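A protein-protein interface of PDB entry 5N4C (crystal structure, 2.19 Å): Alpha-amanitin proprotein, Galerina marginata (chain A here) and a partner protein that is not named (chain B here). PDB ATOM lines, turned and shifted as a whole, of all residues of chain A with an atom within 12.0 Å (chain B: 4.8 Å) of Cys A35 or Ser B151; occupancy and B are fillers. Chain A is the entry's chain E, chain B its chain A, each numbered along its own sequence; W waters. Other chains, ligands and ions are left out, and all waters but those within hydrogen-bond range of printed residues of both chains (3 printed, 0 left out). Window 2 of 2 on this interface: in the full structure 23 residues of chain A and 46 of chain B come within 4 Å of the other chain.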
ATOM      1  N   ALA A  29     -36.679   8.167  -4.215  1.00  0.00           N
ATOM      2  CA  ALA A  29     -36.344   6.783  -3.793  1.00  0.00           C
ATOM      3  C   ALA A  29     -34.841   6.458  -3.791  1.00  0.00           C
ATOM      4  O   ALA A  29     -34.440   5.397  -3.301  1.00  0.00           O
ATOM      5  CB  ALA A  29     -37.089   5.779  -4.663  1.00  0.00           C
ATOM      6  N   SER A  30     -34.013   7.376  -4.285  1.00  0.00           N
ATOM      7  CA  SER A  30     -32.581   7.109  -4.508  1.00  0.00           C
ATOM      8  C   SER A  30     -31.780   6.824  -3.244  1.00  0.00           C
ATOM      9  O   SER A  30     -30.672   6.303  -3.330  1.00  0.00           O
ATOM     10  CB  SER A  30     -31.912   8.268  -5.293  1.00  0.00           C
ATOM     11  OG  SER A  30     -31.931   9.485  -4.552  1.00  0.00           O
ATOM     12  N   GLY A  31     -32.326   7.173  -2.085  1.00  0.00           N
ATOM     13  CA  GLY A  31     -31.686   6.892  -0.805  1.00  0.00           C
ATOM     14  C   GLY A  31     -32.155   5.622  -0.104  1.00  0.00           C
ATOM     15  O   GLY A  31     -31.683   5.328   1.002  1.00  0.00           O
ATOM     16  N   ASN A  32     -33.064   4.859  -0.729  1.00  0.00           N
ATOM     17  CA  ASN A  32     -33.705   3.717  -0.049  1.00  0.00           C
ATOM     18  C   ASN A  32     -32.784   2.524   0.281  1.00  0.00           C
ATOM     19  O   ASN A  32     -33.023   1.821   1.259  1.00  0.00           O
ATOM     20  CB  ASN A  32     -34.932   3.230  -0.841  1.00  0.00           C
ATOM     21  CG  ASN A  32     -36.118   4.181  -0.735  1.00  0.00           C
ATOM     22  OD1 ASN A  32     -36.060   5.216  -0.044  1.00  0.00           O
ATOM     23  ND2 ASN A  32     -37.196   3.842  -1.430  1.00  0.00           N
ATOM     24  N   ASP A  33     -31.745   2.285  -0.521  1.00  0.00           N
ATOM     25  CA  ASP A  33     -30.844   1.137  -0.306  1.00  0.00           C
ATOM     26  C   ASP A  33     -29.357   1.502  -0.563  1.00  0.00           C
ATOM     27  O   ASP A  33     -28.724   0.954  -1.477  1.00  0.00           O
ATOM     28  CB  ASP A  33     -31.320   0.008  -1.218  1.00  0.00           C
ATOM     29  CG  ASP A  33     -30.628  -1.359  -0.941  1.00  0.00           C
ATOM     30  OD1 ASP A  33     -30.217  -1.650   0.206  1.00  0.00           O
ATOM     31  OD2 ASP A  33     -30.509  -2.142  -1.913  1.00  0.00           O
ATOM     32  N   ILE A  34     -28.807   2.454   0.221  1.00  0.00           N
ATOM     33  CA  ILE A  34     -27.398   2.874   0.053  1.00  0.00           C
ATOM     34  C   ILE A  34     -26.421   2.360   1.129  1.00  0.00           C
ATOM     35  O   ILE A  34     -25.223   2.646   1.056  1.00  0.00           O
ATOM     36  CB  ILE A  34     -27.225   4.411  -0.140  1.00  0.00           C
ATOM     37  CG1 ILE A  34     -27.703   5.195   1.083  1.00  0.00           C
ATOM     38  CG2 ILE A  34     -27.894   4.860  -1.427  1.00  0.00           C
ATOM     39  CD1 ILE A  34     -27.449   6.677   0.963  1.00  0.00           C
ATOM     40  N   CYS A  35     -26.921   1.632   2.127  1.00  0.00           N
ATOM     41  CA  CYS A  35     -26.062   0.913   3.090  1.00  0.00           C
ATOM     42  C   CYS A  35     -26.724  -0.396   3.565  1.00  0.00           C
ATOM     43  O   CYS A  35     -27.852  -0.366   4.099  1.00  0.00           O
ATOM     44  CB  CYS A  35     -25.743   1.770   4.321  1.00  0.00           C
ATOM     45  SG  CYS A  35     -24.480   1.056   5.410  1.00  0.00           S
ATOM     46  OXT CYS A  35     -26.110  -1.483   3.448  1.00  0.00           O
ATOM     47  N   THR B  88     -30.253   8.215   5.461  1.00  0.00           N
ATOM     48  CA  THR B  88     -29.731   6.950   6.036  1.00  0.00           C
ATOM     49  C   THR B  88     -28.700   7.254   7.131  1.00  0.00           C
ATOM     50  O   THR B  88     -27.784   8.053   6.931  1.00  0.00           O
ATOM     51  CB  THR B  88     -29.061   6.078   4.945  1.00  0.00           C
ATOM     52  OG1 THR B  88     -29.996   5.839   3.887  1.00  0.00           O
ATOM     53  CG2 THR B  88     -28.626   4.734   5.474  1.00  0.00           C
ATOM     54  N   LEU B  90     -25.601   6.047   9.158  1.00  0.00           N
ATOM     55  CA  LEU B  90     -24.471   5.116   9.123  1.00  0.00           C
ATOM     56  C   LEU B  90     -23.876   4.995  10.532  1.00  0.00           C
ATOM     57  O   LEU B  90     -24.235   5.765  11.431  1.00  0.00           O
ATOM     58  CB  LEU B  90     -23.397   5.608   8.157  1.00  0.00           C
ATOM     59  CG  LEU B  90     -23.776   6.038   6.740  1.00  0.00           C
ATOM     60  CD1 LEU B  90     -22.507   6.446   5.996  1.00  0.00           C
ATOM     61  CD2 LEU B  90     -24.498   4.958   5.965  1.00  0.00           C
ATOM     62  N   LYS B 149     -23.001   2.283  -2.844  1.00  0.00           N
ATOM     63  CA  LYS B 149     -23.220   1.594  -1.563  1.00  0.00           C
ATOM     64  C   LYS B 149     -22.154   1.879  -0.526  1.00  0.00           C
ATOM     65  O   LYS B 149     -20.982   1.629  -0.789  1.00  0.00           O
ATOM     66  CB  LYS B 149     -23.371   0.066  -1.719  1.00  0.00           C
ATOM     67  CG  LYS B 149     -24.816  -0.152  -1.223  1.00  0.00           C
ATOM     68  CD  LYS B 149     -25.365  -1.544  -1.186  1.00  0.00           C
ATOM     69  CE  LYS B 149     -26.731  -1.674  -1.855  1.00  0.00           C
ATOM     70  NZ  LYS B 149     -27.066  -3.111  -2.062  1.00  0.00           N
ATOM     71  N   PHE B 150     -22.560   2.385   0.646  1.00  0.00           N
ATOM     72  CA  PHE B 150     -21.667   2.502   1.795  1.00  0.00           C
ATOM     73  C   PHE B 150     -21.427   1.115   2.373  1.00  0.00           C
ATOM     74  O   PHE B 150     -22.348   0.286   2.391  1.00  0.00           O
ATOM     75  CB  PHE B 150     -22.276   3.371   2.902  1.00  0.00           C
ATOM     76  CG  PHE B 150     -22.263   4.869   2.615  1.00  0.00           C
ATOM     77  CD1 PHE B 150     -21.105   5.615   2.771  1.00  0.00           C
ATOM     78  CD2 PHE B 150     -23.432   5.530   2.241  1.00  0.00           C
ATOM     79  CE1 PHE B 150     -21.104   6.994   2.544  1.00  0.00           C
ATOM     80  CE2 PHE B 150     -23.448   6.900   2.021  1.00  0.00           C
ATOM     81  CZ  PHE B 150     -22.284   7.628   2.168  1.00  0.00           C
ATOM     82  N   SER B 151     -20.214   0.882   2.878  1.00  0.00           N
ATOM     83  CA  SER B 151     -19.917  -0.313   3.672  1.00  0.00           C
ATOM     84  C   SER B 151     -20.739  -0.339   4.992  1.00  0.00           C
ATOM     85  O   SER B 151     -21.135   0.702   5.483  1.00  0.00           O
ATOM     86  CB  SER B 151     -18.422  -0.380   3.975  1.00  0.00           C
ATOM     87  OG  SER B 151     -18.022   0.663   4.843  1.00  0.00           O
ATOM     88  N   PRO B 152     -20.991  -1.532   5.558  1.00  0.00           N
ATOM     89  CA  PRO B 152     -21.737  -1.646   6.821  1.00  0.00           C
ATOM     90  C   PRO B 152     -21.169  -0.854   7.983  1.00  0.00           C
ATOM     91  O   PRO B 152     -21.931  -0.268   8.764  1.00  0.00           O
ATOM     92  CB  PRO B 152     -21.686  -3.157   7.115  1.00  0.00           C
ATOM     93  CG  PRO B 152     -21.670  -3.771   5.761  1.00  0.00           C
ATOM     94  CD  PRO B 152     -20.834  -2.860   4.911  1.00  0.00           C
ATOM     95  N   ASP B 153     -19.846  -0.811   8.093  1.00  0.00           N
ATOM     96  CA  ASP B 153     -19.210  -0.010   9.148  1.00  0.00           C
ATOM     97  C   ASP B 153     -19.168   1.503   8.859  1.00  0.00           C
ATOM     98  O   ASP B 153     -18.706   2.257   9.700  1.00  0.00           O
ATOM     99  CB  ASP B 153     -17.810  -0.554   9.499  1.00  0.00           C
ATOM    100  CG  ASP B 153     -16.750  -0.326   8.389  1.00  0.00           C
ATOM    101  OD1 ASP B 153     -17.018   0.302   7.327  1.00  0.00           O
ATOM    102  OD2 ASP B 153     -15.620  -0.794   8.604  1.00  0.00           O
ATOM    103  N   GLY B 154     -19.613   1.932   7.680  1.00  0.00           N
ATOM    104  CA  GLY B 154     -19.687   3.351   7.332  1.00  0.00           C
ATOM    105  C   GLY B 154     -18.382   4.003   6.905  1.00  0.00           C
ATOM    106  O   GLY B 154     -18.384   5.199   6.563  1.00  0.00           O
ATOM    107  N   LYS B 155     -17.280   3.252   6.846  1.00  0.00           N
ATOM    108  CA  LYS B 155     -15.951   3.828   6.580  1.00  0.00           C
ATOM    109  C   LYS B 155     -15.592   3.982   5.099  1.00  0.00           C
ATOM    110  O   LYS B 155     -14.692   4.746   4.772  1.00  0.00           O
ATOM    111  CB  LYS B 155     -14.850   3.009   7.275  1.00  0.00           C
ATOM    112  CG  LYS B 155     -15.017   2.973   8.783  1.00  0.00           C
ATOM    113  CD  LYS B 155     -13.997   2.181   9.564  1.00  0.00           C
ATOM    114  CE  LYS B 155     -14.255   2.427  11.056  1.00  0.00           C
ATOM    115  NZ  LYS B 155     -14.184   1.181  11.881  1.00  0.00           N
ATOM    116  N   PHE B 156     -16.300   3.289   4.205  1.00  0.00           N
ATOM    117  CA  PHE B 156     -16.002   3.346   2.780  1.00  0.00           C
ATOM    118  C   PHE B 156     -17.262   3.552   1.963  1.00  0.00           C
ATOM    119  O   PHE B 156     -18.346   3.201   2.398  1.00  0.00           O
ATOM    120  CB  PHE B 156     -15.264   2.068   2.345  1.00  0.00           C
ATOM    121  CG  PHE B 156     -13.858   1.972   2.884  1.00  0.00           C
ATOM    122  CD1 PHE B 156     -12.885   2.871   2.476  1.00  0.00           C
ATOM    123  CD2 PHE B 156     -13.515   0.989   3.806  1.00  0.00           C
ATOM    124  CE1 PHE B 156     -11.592   2.804   2.990  1.00  0.00           C
ATOM    125  CE2 PHE B 156     -12.235   0.919   4.325  1.00  0.00           C
ATOM    126  CZ  PHE B 156     -11.274   1.830   3.927  1.00  0.00           C
ATOM    127  N   TRP B 207     -21.769  -5.621  -0.126  1.00  0.00           N
ATOM    128  CA  TRP B 207     -20.695  -5.717   0.853  1.00  0.00           C
ATOM    129  C   TRP B 207     -20.836  -6.939   1.739  1.00  0.00           C
ATOM    130  O   TRP B 207     -21.953  -7.327   2.044  1.00  0.00           O
ATOM    131  CB  TRP B 207     -20.659  -4.469   1.751  1.00  0.00           C
ATOM    132  CG  TRP B 207     -20.175  -3.186   1.092  1.00  0.00           C
ATOM    133  CD1 TRP B 207     -20.937  -2.284   0.421  1.00  0.00           C
ATOM    134  CD2 TRP B 207     -18.834  -2.679   1.077  1.00  0.00           C
ATOM    135  NE1 TRP B 207     -20.157  -1.248  -0.029  1.00  0.00           N
ATOM    136  CE2 TRP B 207     -18.859  -1.460   0.360  1.00  0.00           C
ATOM    137  CE3 TRP B 207     -17.610  -3.136   1.599  1.00  0.00           C
ATOM    138  CZ2 TRP B 207     -17.706  -0.682   0.144  1.00  0.00           C
ATOM    139  CZ3 TRP B 207     -16.454  -2.350   1.391  1.00  0.00           C
ATOM    140  CH2 TRP B 207     -16.522  -1.134   0.667  1.00  0.00           C
ATOM    141  N   SER B 211     -17.076  -5.632   6.210  1.00  0.00           N
ATOM    142  CA  SER B 211     -16.648  -4.401   5.506  1.00  0.00           C
ATOM    143  C   SER B 211     -15.278  -4.468   4.800  1.00  0.00           C
ATOM    144  O   SER B 211     -14.737  -3.429   4.424  1.00  0.00           O
ATOM    145  CB  SER B 211     -16.718  -3.178   6.441  1.00  0.00           C
ATOM    146  OG  SER B 211     -18.057  -2.938   6.860  1.00  0.00           O
ATOM    147  N   ARG B 410     -32.366  -0.047   7.859  1.00  0.00           N
ATOM    148  CA  ARG B 410     -31.327  -1.042   8.155  1.00  0.00           C
ATOM    149  C   ARG B 410     -31.825  -1.892   9.317  1.00  0.00           C
ATOM    150  O   ARG B 410     -32.232  -1.357  10.355  1.00  0.00           O
ATOM    151  CB  ARG B 410     -29.972  -0.395   8.492  1.00  0.00           C
ATOM    152  CG  ARG B 410     -29.435   0.556   7.426  1.00  0.00           C
ATOM    153  CD  ARG B 410     -28.152   1.255   7.910  1.00  0.00           C
ATOM    154  NE  ARG B 410     -27.025   0.331   8.050  1.00  0.00           N
ATOM    155  CZ  ARG B 410     -25.911   0.551   8.758  1.00  0.00           C
ATOM    156  NH1 ARG B 410     -25.700   1.705   9.413  1.00  0.00           N
ATOM    157  NH2 ARG B 410     -24.972  -0.410   8.798  1.00  0.00           N
HETATM  158  O   HOH W   1     -30.303   3.660   2.719  1.00  0.00           O
HETATM  159  O   HOH W   2     -23.808  -2.171   2.753  1.00  0.00           O
HETATM  160  O   HOH W   3     -30.407   7.878   2.237  1.00  0.00           O
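Among the printed residues, pairs that only touch across the chains: Ile A34 with Lys B149 (3.5 Å), Ile A34 with Thr B88 (3.7 Å) and Cys A35 with Leu B90 (3.8 Å).
The guanidinium group (NH2) of Arg B410 is in hydrogen-bond range of the backbone carbonyl oxygen (O) of Pro B152 (3.0 Å). The side-chain hydroxyl of Ser B151 is in hydrogen-bond range of the backbone NH of Gly B154 (3.5 Å). The indole nitrogen (NE1) of Trp B207 lies within hydrogen-bond range of the backbone carbonyl oxygen (O) of Lys B149 (3.1 Å). N of Ser B151 sits at hydrogen-bond distance from O of Phe B156, 3.0 Å away. N of Lys B155 is in hydrogen-bond range of OG of Ser B151, at 3.4 Å. The side-chain hydroxyl (OG) of Ser B151 sits at hydrogen-bond distance from the side-chain carboxylate (OD1) of Asp B153 (2.7 Å).
Printed residues of chain B within 4 Å of Cys A35: Leu B90, Phe B150, Ser B151 and Arg B410. Ser B151 touches just one residue of chain A: Cys A35. Of chain A, only Gly A31 (3.4 Å) and Ile A34 (3.7 Å) come within 4 Å of Thr B88. Phe B150 touches just these residues of chain A: Ile A34 (2.7 Å) and Cys A35 (3.8 Å). No residue of chain A comes within 4 Å of Pro B152. No residue of chain A comes within 4 Å of Asp B153. Gly B154 touches none of the printed residues of chain A. No residue of chain A comes within 4 Å of Phe B156. Trp B207 touches none of the printed residues of chain A. No residue of chain A comes within 4 Å of Ser B211. Of chain A, only Cys A35 (3.7 Å) comes within 4 Å of Arg B410. Of the printed residues of chain B, Gly A31 touches Thr B88 (3.4 Å). Of the printed residues of chain B, Asp A33 touches Lys B149 (3.3 Å). Printed residues of chain B within 4 Å of Ile A34: Thr B88 (3.7 Å), Lys B149 (3.5 Å) and Phe B150 (2.7 Å). Asn A32 touches none of the printed residues of chain B. Lys B155 touches none of the printed residues of chain A. The nearest printed residue of chain B that does not touch Asp A33 is Thr B88 (5.9 Å).
N of Phe B150 lies within hydrogen-bond range of O of Ile A34 (2.7 Å). The backbone carbonyl oxygen of Gly A31 lies within hydrogen-bond range of the side-chain hydroxyl of Thr B88 (3.4 Å). The side-chain carboxylate (OD2) of Asp A33 is in salt-bridge range of the side-chain amino group (NZ) of Lys B149, at 3.6 Å. The backbone carbonyl oxygen of Ser B151 is in hydrogen-bond range of the side-chain sulfur of Cys A35 (3.4 Å). The guanidinium group of Arg B410 lies close to the side-chain sulfur of Cys A35 (3.7 Å). The side-chain sulfur (SG) of Cys A35 sits at hydrogen-bond distance from the backbone carbonyl oxygen (O) of Phe B150.
Hydrophobic or aromatic side chains of chain A within 4 Å of the printed part of chain B: Ile A34. Of the 13 printed residues of chain B, 6 touch a printed residue of chain A. Among the printed residues, 9 pairs touch across the chains.
Water W1 lies within hydrogen-bond range of OG1 of Thr B88 (2.5 Å), O of Gly A31 (2.8 Å) and N of Ile A34 (3.2 Å). Water W2 bridges the chain-end carboxylate of Cys A35 and the backbone carbonyl oxygen of Phe B150. Water W3 bridges the side-chain hydroxyl (OG1) of Thr B88 (2.7 Å) and the backbone carbonyl oxygen (O) of Gly A31 (3.1 Å).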
